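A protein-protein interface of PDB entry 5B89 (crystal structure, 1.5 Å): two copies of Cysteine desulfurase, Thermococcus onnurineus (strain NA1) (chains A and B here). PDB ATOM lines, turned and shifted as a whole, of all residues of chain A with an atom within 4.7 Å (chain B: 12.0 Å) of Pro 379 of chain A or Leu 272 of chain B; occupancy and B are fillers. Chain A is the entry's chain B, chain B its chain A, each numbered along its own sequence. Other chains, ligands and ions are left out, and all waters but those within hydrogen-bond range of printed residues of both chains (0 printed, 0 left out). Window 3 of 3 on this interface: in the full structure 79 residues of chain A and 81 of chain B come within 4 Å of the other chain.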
ATOM      1  N   PRO A 131       3.604  15.245 -18.456  1.00  0.00           N
ATOM      2  CA  PRO A 131       2.930  15.596 -17.232  1.00  0.00           C
ATOM      3  C   PRO A 131       3.894  15.952 -16.153  1.00  0.00           C
ATOM      4  O   PRO A 131       3.454  16.113 -15.065  1.00  0.00           O
ATOM      5  CB  PRO A 131       2.250  14.308 -16.808  1.00  0.00           C
ATOM      6  CG  PRO A 131       3.050  13.246 -17.414  1.00  0.00           C
ATOM      7  CD  PRO A 131       3.680  13.801 -18.658  1.00  0.00           C
ATOM      8  N   HIS A 135       6.756  24.458 -14.006  1.00  0.00           N
ATOM      9  CA  HIS A 135       5.709  25.437 -14.301  1.00  0.00           C
ATOM     10  C   HIS A 135       6.093  26.333 -15.475  1.00  0.00           C
ATOM     11  O   HIS A 135       5.180  26.803 -16.225  1.00  0.00           O
ATOM     12  CB  HIS A 135       5.375  26.249 -13.105  1.00  0.00           C
ATOM     13  CG  HIS A 135       4.834  25.415 -11.958  1.00  0.00           C
ATOM     14  ND1 HIS A 135       4.979  25.783 -10.638  1.00  0.00           N
ATOM     15  CD2 HIS A 135       4.257  24.202 -11.969  1.00  0.00           C
ATOM     16  CE1 HIS A 135       4.428  24.832  -9.864  1.00  0.00           C
ATOM     17  NE2 HIS A 135       4.045  23.839 -10.639  1.00  0.00           N
ATOM     18  N   LEU A 138       4.937  24.857 -18.658  1.00  0.00           N
ATOM     19  CA  LEU A 138       3.548  24.442 -18.612  1.00  0.00           C
ATOM     20  C   LEU A 138       2.614  25.624 -18.755  1.00  0.00           C
ATOM     21  O   LEU A 138       1.834  25.650 -19.646  1.00  0.00           O
ATOM     22  CB  LEU A 138       3.278  23.693 -17.324  1.00  0.00           C
ATOM     23  CG  LEU A 138       1.842  23.289 -17.119  1.00  0.00           C
ATOM     24  CD1 LEU A 138       1.392  22.477 -18.293  1.00  0.00           C
ATOM     25  CD2 LEU A 138       1.670  22.509 -15.846  1.00  0.00           C
ATOM     26  N   GLN A 142      -0.528  26.455 -21.261  1.00  0.00           N
ATOM     27  CA  GLN A 142      -1.904  26.550 -20.694  1.00  0.00           C
ATOM     28  C   GLN A 142      -2.563  27.805 -21.031  1.00  0.00           C
ATOM     29  O   GLN A 142      -3.780  27.794 -21.393  1.00  0.00           O
ATOM     30  CB  GLN A 142      -1.863  26.377 -19.172  1.00  0.00           C
ATOM     31  CG  GLN A 142      -1.563  24.982 -18.728  1.00  0.00           C
ATOM     32  CD  GLN A 142      -1.419  24.909 -17.212  1.00  0.00           C
ATOM     33  OE1 GLN A 142      -0.914  25.865 -16.599  1.00  0.00           O
ATOM     34  NE2 GLN A 142      -1.775  23.819 -16.633  1.00  0.00           N
ATOM     35  N   PHE A 154      -1.221  15.620 -22.710  1.00  0.00           N
ATOM     36  CA  PHE A 154      -0.087  15.193 -21.968  1.00  0.00           C
ATOM     37  C   PHE A 154       0.236  13.773 -22.244  1.00  0.00           C
ATOM     38  O   PHE A 154      -0.690  12.856 -22.136  1.00  0.00           O
ATOM     39  CB  PHE A 154      -0.406  15.315 -20.464  1.00  0.00           C
ATOM     40  CG  PHE A 154      -0.740  16.691 -20.053  1.00  0.00           C
ATOM     41  CD1 PHE A 154       0.262  17.665 -19.868  1.00  0.00           C
ATOM     42  CD2 PHE A 154      -2.029  17.078 -20.008  1.00  0.00           C
ATOM     43  CE1 PHE A 154      -0.037  18.944 -19.592  1.00  0.00           C
ATOM     44  CE2 PHE A 154      -2.364  18.353 -19.697  1.00  0.00           C
ATOM     45  CZ  PHE A 154      -1.387  19.304 -19.477  1.00  0.00           C
ATOM     46  N   ALA A 377       6.897  22.098  -9.612  1.00  0.00           N
ATOM     47  CA  ALA A 377       6.449  20.994 -10.419  1.00  0.00           C
ATOM     48  C   ALA A 377       5.283  20.329  -9.705  1.00  0.00           C
ATOM     49  O   ALA A 377       5.335  19.137  -9.377  1.00  0.00           O
ATOM     50  CB  ALA A 377       7.537  20.027 -10.689  1.00  0.00           C
ATOM     51  N   LEU A 378       4.273  21.157  -9.437  1.00  0.00           N
ATOM     52  CA  LEU A 378       3.071  20.639  -8.698  1.00  0.00           C
ATOM     53  C   LEU A 378       2.373  19.473  -9.338  1.00  0.00           C
ATOM     54  O   LEU A 378       1.917  18.539  -8.589  1.00  0.00           O
ATOM     55  CB  LEU A 378       2.110  21.766  -8.333  1.00  0.00           C
ATOM     56  CG  LEU A 378       2.514  22.650  -7.145  1.00  0.00           C
ATOM     57  CD1 LEU A 378       1.826  24.016  -6.956  1.00  0.00           C
ATOM     58  CD2 LEU A 378       2.182  21.887  -5.831  1.00  0.00           C
ATOM     59  N   PRO A 379       2.292  19.396 -10.641  1.00  0.00           N
ATOM     60  CA  PRO A 379       1.616  18.237 -11.207  1.00  0.00           C
ATOM     61  C   PRO A 379       2.368  16.957 -10.953  1.00  0.00           C
ATOM     62  O   PRO A 379       1.733  15.957 -10.901  1.00  0.00           O
ATOM     63  CB  PRO A 379       1.495  18.576 -12.673  1.00  0.00           C
ATOM     64  CG  PRO A 379       1.303  20.058 -12.634  1.00  0.00           C
ATOM     65  CD  PRO A 379       2.360  20.490 -11.625  1.00  0.00           C
ATOM     66  N   VAL A 380       3.681  17.014 -10.781  1.00  0.00           N
ATOM     67  CA  VAL A 380       4.450  15.831 -10.447  1.00  0.00           C
ATOM     68  C   VAL A 380       4.017  15.355  -9.035  1.00  0.00           C
ATOM     69  O   VAL A 380       3.800  14.213  -8.807  1.00  0.00           O
ATOM     70  CB  VAL A 380       5.983  16.083 -10.449  1.00  0.00           C
ATOM     71  CG1 VAL A 380       6.734  14.946  -9.789  1.00  0.00           C
ATOM     72  CG2 VAL A 380       6.505  16.269 -11.865  1.00  0.00           C
ATOM     73  N   MET A 381       3.937  16.286  -8.117  1.00  0.00           N
ATOM     74  CA  MET A 381       3.566  15.958  -6.758  1.00  0.00           C
ATOM     75  C   MET A 381       2.149  15.421  -6.729  1.00  0.00           C
ATOM     76  O   MET A 381       1.867  14.453  -6.104  1.00  0.00           O
ATOM     77  CB  MET A 381       3.730  17.140  -5.832  1.00  0.00           C
ATOM     78  CG  MET A 381       5.098  17.778  -5.853  1.00  0.00           C
ATOM     79  SD  MET A 381       6.414  16.591  -5.526  1.00  0.00           S
ATOM     80  CE  MET A 381       7.813  17.334  -6.418  1.00  0.00           C
ATOM     81  N   LYS A 382       1.282  16.077  -7.455  1.00  0.00           N
ATOM     82  CA  LYS A 382      -0.129  15.647  -7.441  1.00  0.00           C
ATOM     83  C   LYS A 382      -0.274  14.264  -8.104  1.00  0.00           C
ATOM     84  O   LYS A 382      -1.028  13.428  -7.578  1.00  0.00           O
ATOM     85  CB  LYS A 382      -0.984  16.711  -8.086  1.00  0.00           C
ATOM     86  CG  LYS A 382      -1.084  17.941  -7.268  1.00  0.00           C
ATOM     87  CD  LYS A 382      -1.876  19.024  -8.001  1.00  0.00           C
ATOM     88  CE  LYS A 382      -1.795  20.262  -7.182  1.00  0.00           C
ATOM     89  NZ  LYS A 382      -2.676  21.324  -7.771  1.00  0.00           N
ATOM     90  N   LYS A 383       0.507  13.951  -9.141  1.00  0.00           N
ATOM     91  CA  LYS A 383       0.524  12.620  -9.782  1.00  0.00           C
ATOM     92  C   LYS A 383       0.998  11.540  -8.830  1.00  0.00           C
ATOM     93  O   LYS A 383       0.477  10.360  -8.805  1.00  0.00           O
ATOM     94  CB  LYS A 383       1.341  12.655 -11.068  1.00  0.00           C
ATOM     95  CG  LYS A 383       1.429  11.370 -11.876  1.00  0.00           C
ATOM     96  CD  LYS A 383       2.279  11.587 -13.123  1.00  0.00           C
ATOM     97  CE  LYS A 383       2.460  10.381 -13.965  1.00  0.00           C
ATOM     98  NZ  LYS A 383       1.126   9.852 -14.449  1.00  0.00           N
ATOM     99  N   ILE B 262       4.976  34.263 -17.443  1.00  0.00           N
ATOM    100  CA  ILE B 262       4.502  33.482 -16.310  1.00  0.00           C
ATOM    101  C   ILE B 262       5.235  32.153 -16.248  1.00  0.00           C
ATOM    102  O   ILE B 262       5.772  31.566 -17.193  1.00  0.00           O
ATOM    103  CB  ILE B 262       2.970  33.300 -16.395  1.00  0.00           C
ATOM    104  CG1 ILE B 262       2.615  32.639 -17.709  1.00  0.00           C
ATOM    105  CG2 ILE B 262       2.277  34.636 -16.222  1.00  0.00           C
ATOM    106  CD1 ILE B 262       1.133  32.163 -17.737  1.00  0.00           C
ATOM    107  N   GLY B 263       5.278  31.609 -15.042  1.00  0.00           N
ATOM    108  CA  GLY B 263       5.981  30.342 -14.842  1.00  0.00           C
ATOM    109  C   GLY B 263       6.450  30.158 -13.472  1.00  0.00           C
ATOM    110  O   GLY B 263       5.772  30.562 -12.504  1.00  0.00           O
ATOM    111  N   GLY B 264       7.613  29.544 -13.302  1.00  0.00           N
ATOM    112  CA  GLY B 264       8.177  29.369 -11.968  1.00  0.00           C
ATOM    113  C   GLY B 264       8.253  30.677 -11.199  1.00  0.00           C
ATOM    114  O   GLY B 264       8.621  31.678 -11.698  1.00  0.00           O
ATOM    115  N   GLY B 265       7.860  30.606  -9.947  1.00  0.00           N
ATOM    116  CA  GLY B 265       7.883  31.737  -9.062  1.00  0.00           C
ATOM    117  C   GLY B 265       6.657  32.627  -9.094  1.00  0.00           C
ATOM    118  O   GLY B 265       6.521  33.408  -8.240  1.00  0.00           O
ATOM    119  N   ILE B 267       3.333  31.552  -9.246  1.00  0.00           N
ATOM    120  CA  ILE B 267       2.147  30.854  -8.868  1.00  0.00           C
ATOM    121  C   ILE B 267       1.904  30.588  -7.401  1.00  0.00           C
ATOM    122  O   ILE B 267       2.744  30.660  -6.555  1.00  0.00           O
ATOM    123  CB  ILE B 267       2.090  29.460  -9.525  1.00  0.00           C
ATOM    124  CG1 ILE B 267       3.181  28.555  -8.998  1.00  0.00           C
ATOM    125  CG2 ILE B 267       2.262  29.534 -11.027  1.00  0.00           C
ATOM    126  CD1 ILE B 267       2.779  27.772  -7.776  1.00  0.00           C
ATOM    127  N   GLU B 268       0.654  30.250  -7.193  1.00  0.00           N
ATOM    128  CA  GLU B 268       0.175  29.841  -5.917  1.00  0.00           C
ATOM    129  C   GLU B 268      -0.199  28.379  -6.062  1.00  0.00           C
ATOM    130  O   GLU B 268       0.064  27.612  -5.203  1.00  0.00           O
ATOM    131  CB  GLU B 268      -1.005  30.672  -5.519  1.00  0.00           C
ATOM    132  CG  GLU B 268      -1.306  30.518  -4.072  1.00  0.00           C
ATOM    133  CD  GLU B 268      -1.533  31.840  -3.426  1.00  0.00           C
ATOM    134  OE1 GLU B 268      -0.515  32.491  -3.054  1.00  0.00           O
ATOM    135  OE2 GLU B 268      -2.714  32.200  -3.353  1.00  0.00           O
ATOM    136  N   ASP B 269      -0.809  28.010  -7.177  1.00  0.00           N
ATOM    137  CA  ASP B 269      -1.136  26.633  -7.425  1.00  0.00           C
ATOM    138  C   ASP B 269      -1.179  26.335  -8.889  1.00  0.00           C
ATOM    139  O   ASP B 269      -1.486  27.265  -9.652  1.00  0.00           O
ATOM    140  CB  ASP B 269      -2.521  26.332  -6.853  1.00  0.00           C
ATOM    141  CG  ASP B 269      -2.837  24.829  -6.851  1.00  0.00           C
ATOM    142  OD1 ASP B 269      -1.965  23.942  -6.741  1.00  0.00           O
ATOM    143  OD2 ASP B 269      -4.035  24.488  -6.954  1.00  0.00           O
ATOM    144  N   VAL B 270      -0.955  25.069  -9.221  1.00  0.00           N
ATOM    145  CA  VAL B 270      -0.874  24.612 -10.605  1.00  0.00           C
ATOM    146  C   VAL B 270      -1.343  23.176 -10.663  1.00  0.00           C
ATOM    147  O   VAL B 270      -0.951  22.354  -9.833  1.00  0.00           O
ATOM    148  CB  VAL B 270       0.599  24.693 -11.194  1.00  0.00           C
ATOM    149  CG1 VAL B 270       0.633  24.169 -12.620  1.00  0.00           C
ATOM    150  CG2 VAL B 270       1.149  26.073 -11.039  1.00  0.00           C
ATOM    151  N   SER B 271      -2.194  22.838 -11.639  1.00  0.00           N
ATOM    152  CA  SER B 271      -2.509  21.477 -11.967  1.00  0.00           C
ATOM    153  C   SER B 271      -2.372  21.327 -13.487  1.00  0.00           C
ATOM    154  O   SER B 271      -2.077  22.353 -14.173  1.00  0.00           O
ATOM    155  CB  SER B 271      -3.959  21.157 -11.558  1.00  0.00           C
ATOM    156  OG  SER B 271      -4.782  21.988 -12.322  1.00  0.00           O
ATOM    157  N   LEU B 272      -2.523  20.128 -14.020  1.00  0.00           N
ATOM    158  CA  LEU B 272      -2.500  19.940 -15.457  1.00  0.00           C
ATOM    159  C   LEU B 272      -3.557  20.784 -16.172  1.00  0.00           C
ATOM    160  O   LEU B 272      -3.361  21.189 -17.351  1.00  0.00           O
ATOM    161  CB  LEU B 272      -2.607  18.469 -15.858  1.00  0.00           C
ATOM    162  CG  LEU B 272      -1.443  17.610 -15.387  1.00  0.00           C
ATOM    163  CD1 LEU B 272      -1.634  16.166 -15.820  1.00  0.00           C
ATOM    164  CD2 LEU B 272      -0.102  18.200 -15.892  1.00  0.00           C
ATOM    165  N   ASP B 273      -4.684  21.036 -15.453  1.00  0.00           N
ATOM    166  CA  ASP B 273      -5.831  21.767 -15.968  1.00  0.00           C
ATOM    167  C   ASP B 273      -5.705  23.253 -15.877  1.00  0.00           C
ATOM    168  O   ASP B 273      -6.483  23.932 -16.515  1.00  0.00           O
ATOM    169  CB  ASP B 273      -7.119  21.439 -15.149  1.00  0.00           C
ATOM    170  CG  ASP B 273      -7.497  19.979 -15.175  1.00  0.00           C
ATOM    171  OD1 ASP B 273      -6.878  19.161 -15.915  1.00  0.00           O
ATOM    172  OD2 ASP B 273      -8.438  19.647 -14.414  1.00  0.00           O
ATOM    173  N   GLY B 274      -4.802  23.818 -15.064  1.00  0.00           N
ATOM    174  CA  GLY B 274      -4.742  25.282 -14.981  1.00  0.00           C
ATOM    175  C   GLY B 274      -3.832  25.819 -13.884  1.00  0.00           C
ATOM    176  O   GLY B 274      -3.063  25.050 -13.308  1.00  0.00           O
ATOM    177  N   TYR B 275      -3.939  27.113 -13.608  1.00  0.00           N
ATOM    178  CA  TYR B 275      -3.098  27.755 -12.644  1.00  0.00           C
ATOM    179  C   TYR B 275      -3.730  28.915 -11.950  1.00  0.00           C
ATOM    180  O   TYR B 275      -4.678  29.493 -12.446  1.00  0.00           O
ATOM    181  CB  TYR B 275      -1.764  28.155 -13.353  1.00  0.00           C
ATOM    182  CG  TYR B 275      -1.937  29.252 -14.416  1.00  0.00           C
ATOM    183  CD1 TYR B 275      -1.866  30.598 -14.084  1.00  0.00           C
ATOM    184  CD2 TYR B 275      -2.176  28.914 -15.734  1.00  0.00           C
ATOM    185  CE1 TYR B 275      -2.071  31.581 -15.051  1.00  0.00           C
ATOM    186  CE2 TYR B 275      -2.344  29.906 -16.717  1.00  0.00           C
ATOM    187  CZ  TYR B 275      -2.259  31.211 -16.367  1.00  0.00           C
ATOM    188  OH  TYR B 275      -2.446  32.129 -17.312  1.00  0.00           O
ATOM    189  N   LYS B 276      -3.181  29.281 -10.792  1.00  0.00           N
ATOM    190  CA  LYS B 276      -3.526  30.474 -10.027  1.00  0.00           C
ATOM    191  C   LYS B 276      -2.199  31.250  -9.635  1.00  0.00           C
ATOM    192  O   LYS B 276      -1.260  30.666  -9.115  1.00  0.00           O
ATOM    193  CB  LYS B 276      -4.369  30.013  -8.817  1.00  0.00           C
ATOM    194  CG  LYS B 276      -4.589  30.880  -7.627  1.00  0.00           C
ATOM    195  CD  LYS B 276      -4.774  32.326  -7.897  1.00  0.00           C
ATOM    196  CE  LYS B 276      -4.565  33.074  -6.603  1.00  0.00           C
ATOM    197  NZ  LYS B 276      -5.729  32.922  -5.704  1.00  0.00           N
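The side-chain carboxylate (OD1) of Asp 269 of chain B lies within salt-bridge range of the side-chain amino group (NZ) of Lys 382 of chain A (2.9 Å).
The backbone carbonyl oxygen (O) of Val 270 of chain B sits at hydrogen-bond distance from the side-chain amino group (NZ) of Lys 382 of chain A.
The backbone carbonyl oxygen (O) of Ser 271 of chain B lies within hydrogen-bond range of the side-chain amide nitrogen (NE2) of Gln 142 of chain A (2.9 Å).
The side-chain amide nitrogen (NE2) of Gln 142 of chain A is in hydrogen-bond range of the backbone carbonyl oxygen (O) of Leu 272 of chain B (3.2 Å).
The side-chain amide nitrogen (NE2) of Gln 142 of chain A lies close to the backbone NH (N) of Gly 274 of chain B (3.4 Å).
The backbone carbonyl oxygen (O) of Asp 269 of chain B lies within hydrogen-bond range of the backbone NH (N) of Lys 276 of chain B (2.9 Å).
OG of Ser 271 of chain B sits close to N of Asp 273 of chain B, at 3.3 Å.
The side-chain hydroxyl (OG) of Ser 271 of chain B sits at hydrogen-bond distance from the backbone NH (N) of Gly 274 of chain B, at 3.3 Å.
N of Ala 377 of chain A lies within hydrogen-bond range of NE2 of His 135 of chain A (3.5 Å).
A ring nitrogen (NE2) of His 135 of chain A sits at hydrogen-bond distance from the backbone NH (N) of Leu 378 of chain A (2.9 Å).
Among the printed residues, pairs that only touch across the chains: His 135 of chain A with Gly 263 of chain B (3.9 Å), His 135 of chain A with Gly 264 of chain B (3.99 Å), His 135 of chain A with Ile 267 of chain B (3.7 Å), His 135 of chain A with Val 270 of chain B (3.6 Å), Leu 138 of chain A with Val 270 of chain B (3.8 Å), Gln 142 of chain A with Tyr 275 of chain B (3.4 Å), Phe 154 of chain A with Leu 272 of chain B (3.5 Å), Leu 378 of chain A with Ile 267 of chain B (3.96 Å), Leu 378 of chain A with Asp 269 of chain B (3.8 Å), Leu 378 of chain A with Val 270 of chain B (3.5 Å), Pro 379 of chain A with Ser 271 of chain B (3.98 Å) and Pro 379 of chain A with Leu 272 of chain B (3.6 Å).
Of the printed residues of chain B, Pro 379 of chain A touches Ser 271 and Leu 272.
No residue of chain B comes within 4 Å of Pro 131 of chain A.
Phe 154 of chain A touches one residue of chain B.
Ala 377 of chain A touches none of the printed residues of chain B.
Leu 378 of chain A touches just these residues of chain B: Ile 267, Asp 269 and Val 270.
No residue of chain B comes within 4 Å of Val 380 of chain A.
No residue of chain B comes within 4 Å of Lys 383 of chain A.
Of the printed residues of chain A, Gly 264 of chain B touches His 135.
Of the printed residues of chain A, Gly 263 of chain B touches His 135.
Printed residues of chain A within 4 Å of Ser 271 of chain B: Gln 142 and Pro 379.
The nearest printed residue of chain B that does not touch Pro 379 of chain A is Val 270 of chain B (4.2 Å).
The nearest residue of chain A that does not touch Leu 272 of chain B is Pro 131 of chain A (4.2 Å).
The nearest printed residue of chain A that does not touch Gly 274 of chain B is Leu 138 of chain A (5.9 Å).
Printed residues of chain A that touch a printed residue of chain B: His 135, Leu 138, Gln 142, Phe 154, Leu 378, Pro 379 and Lys 382.
Hydrophobic or aromatic side chains of chain A that line the printed part of chain B: His 135, Leu 138, Phe 154, Leu 378 and Pro 379.
Among the printed residues, 17 pairs touch across the chains.
Among the printed residues, Asp or Glu carboxylates within 4 Å of a Lys or Arg side-chain nitrogen of the other chain: Lys 382 of chain A with Asp 269 of chain B.
No position is printed for both chains.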
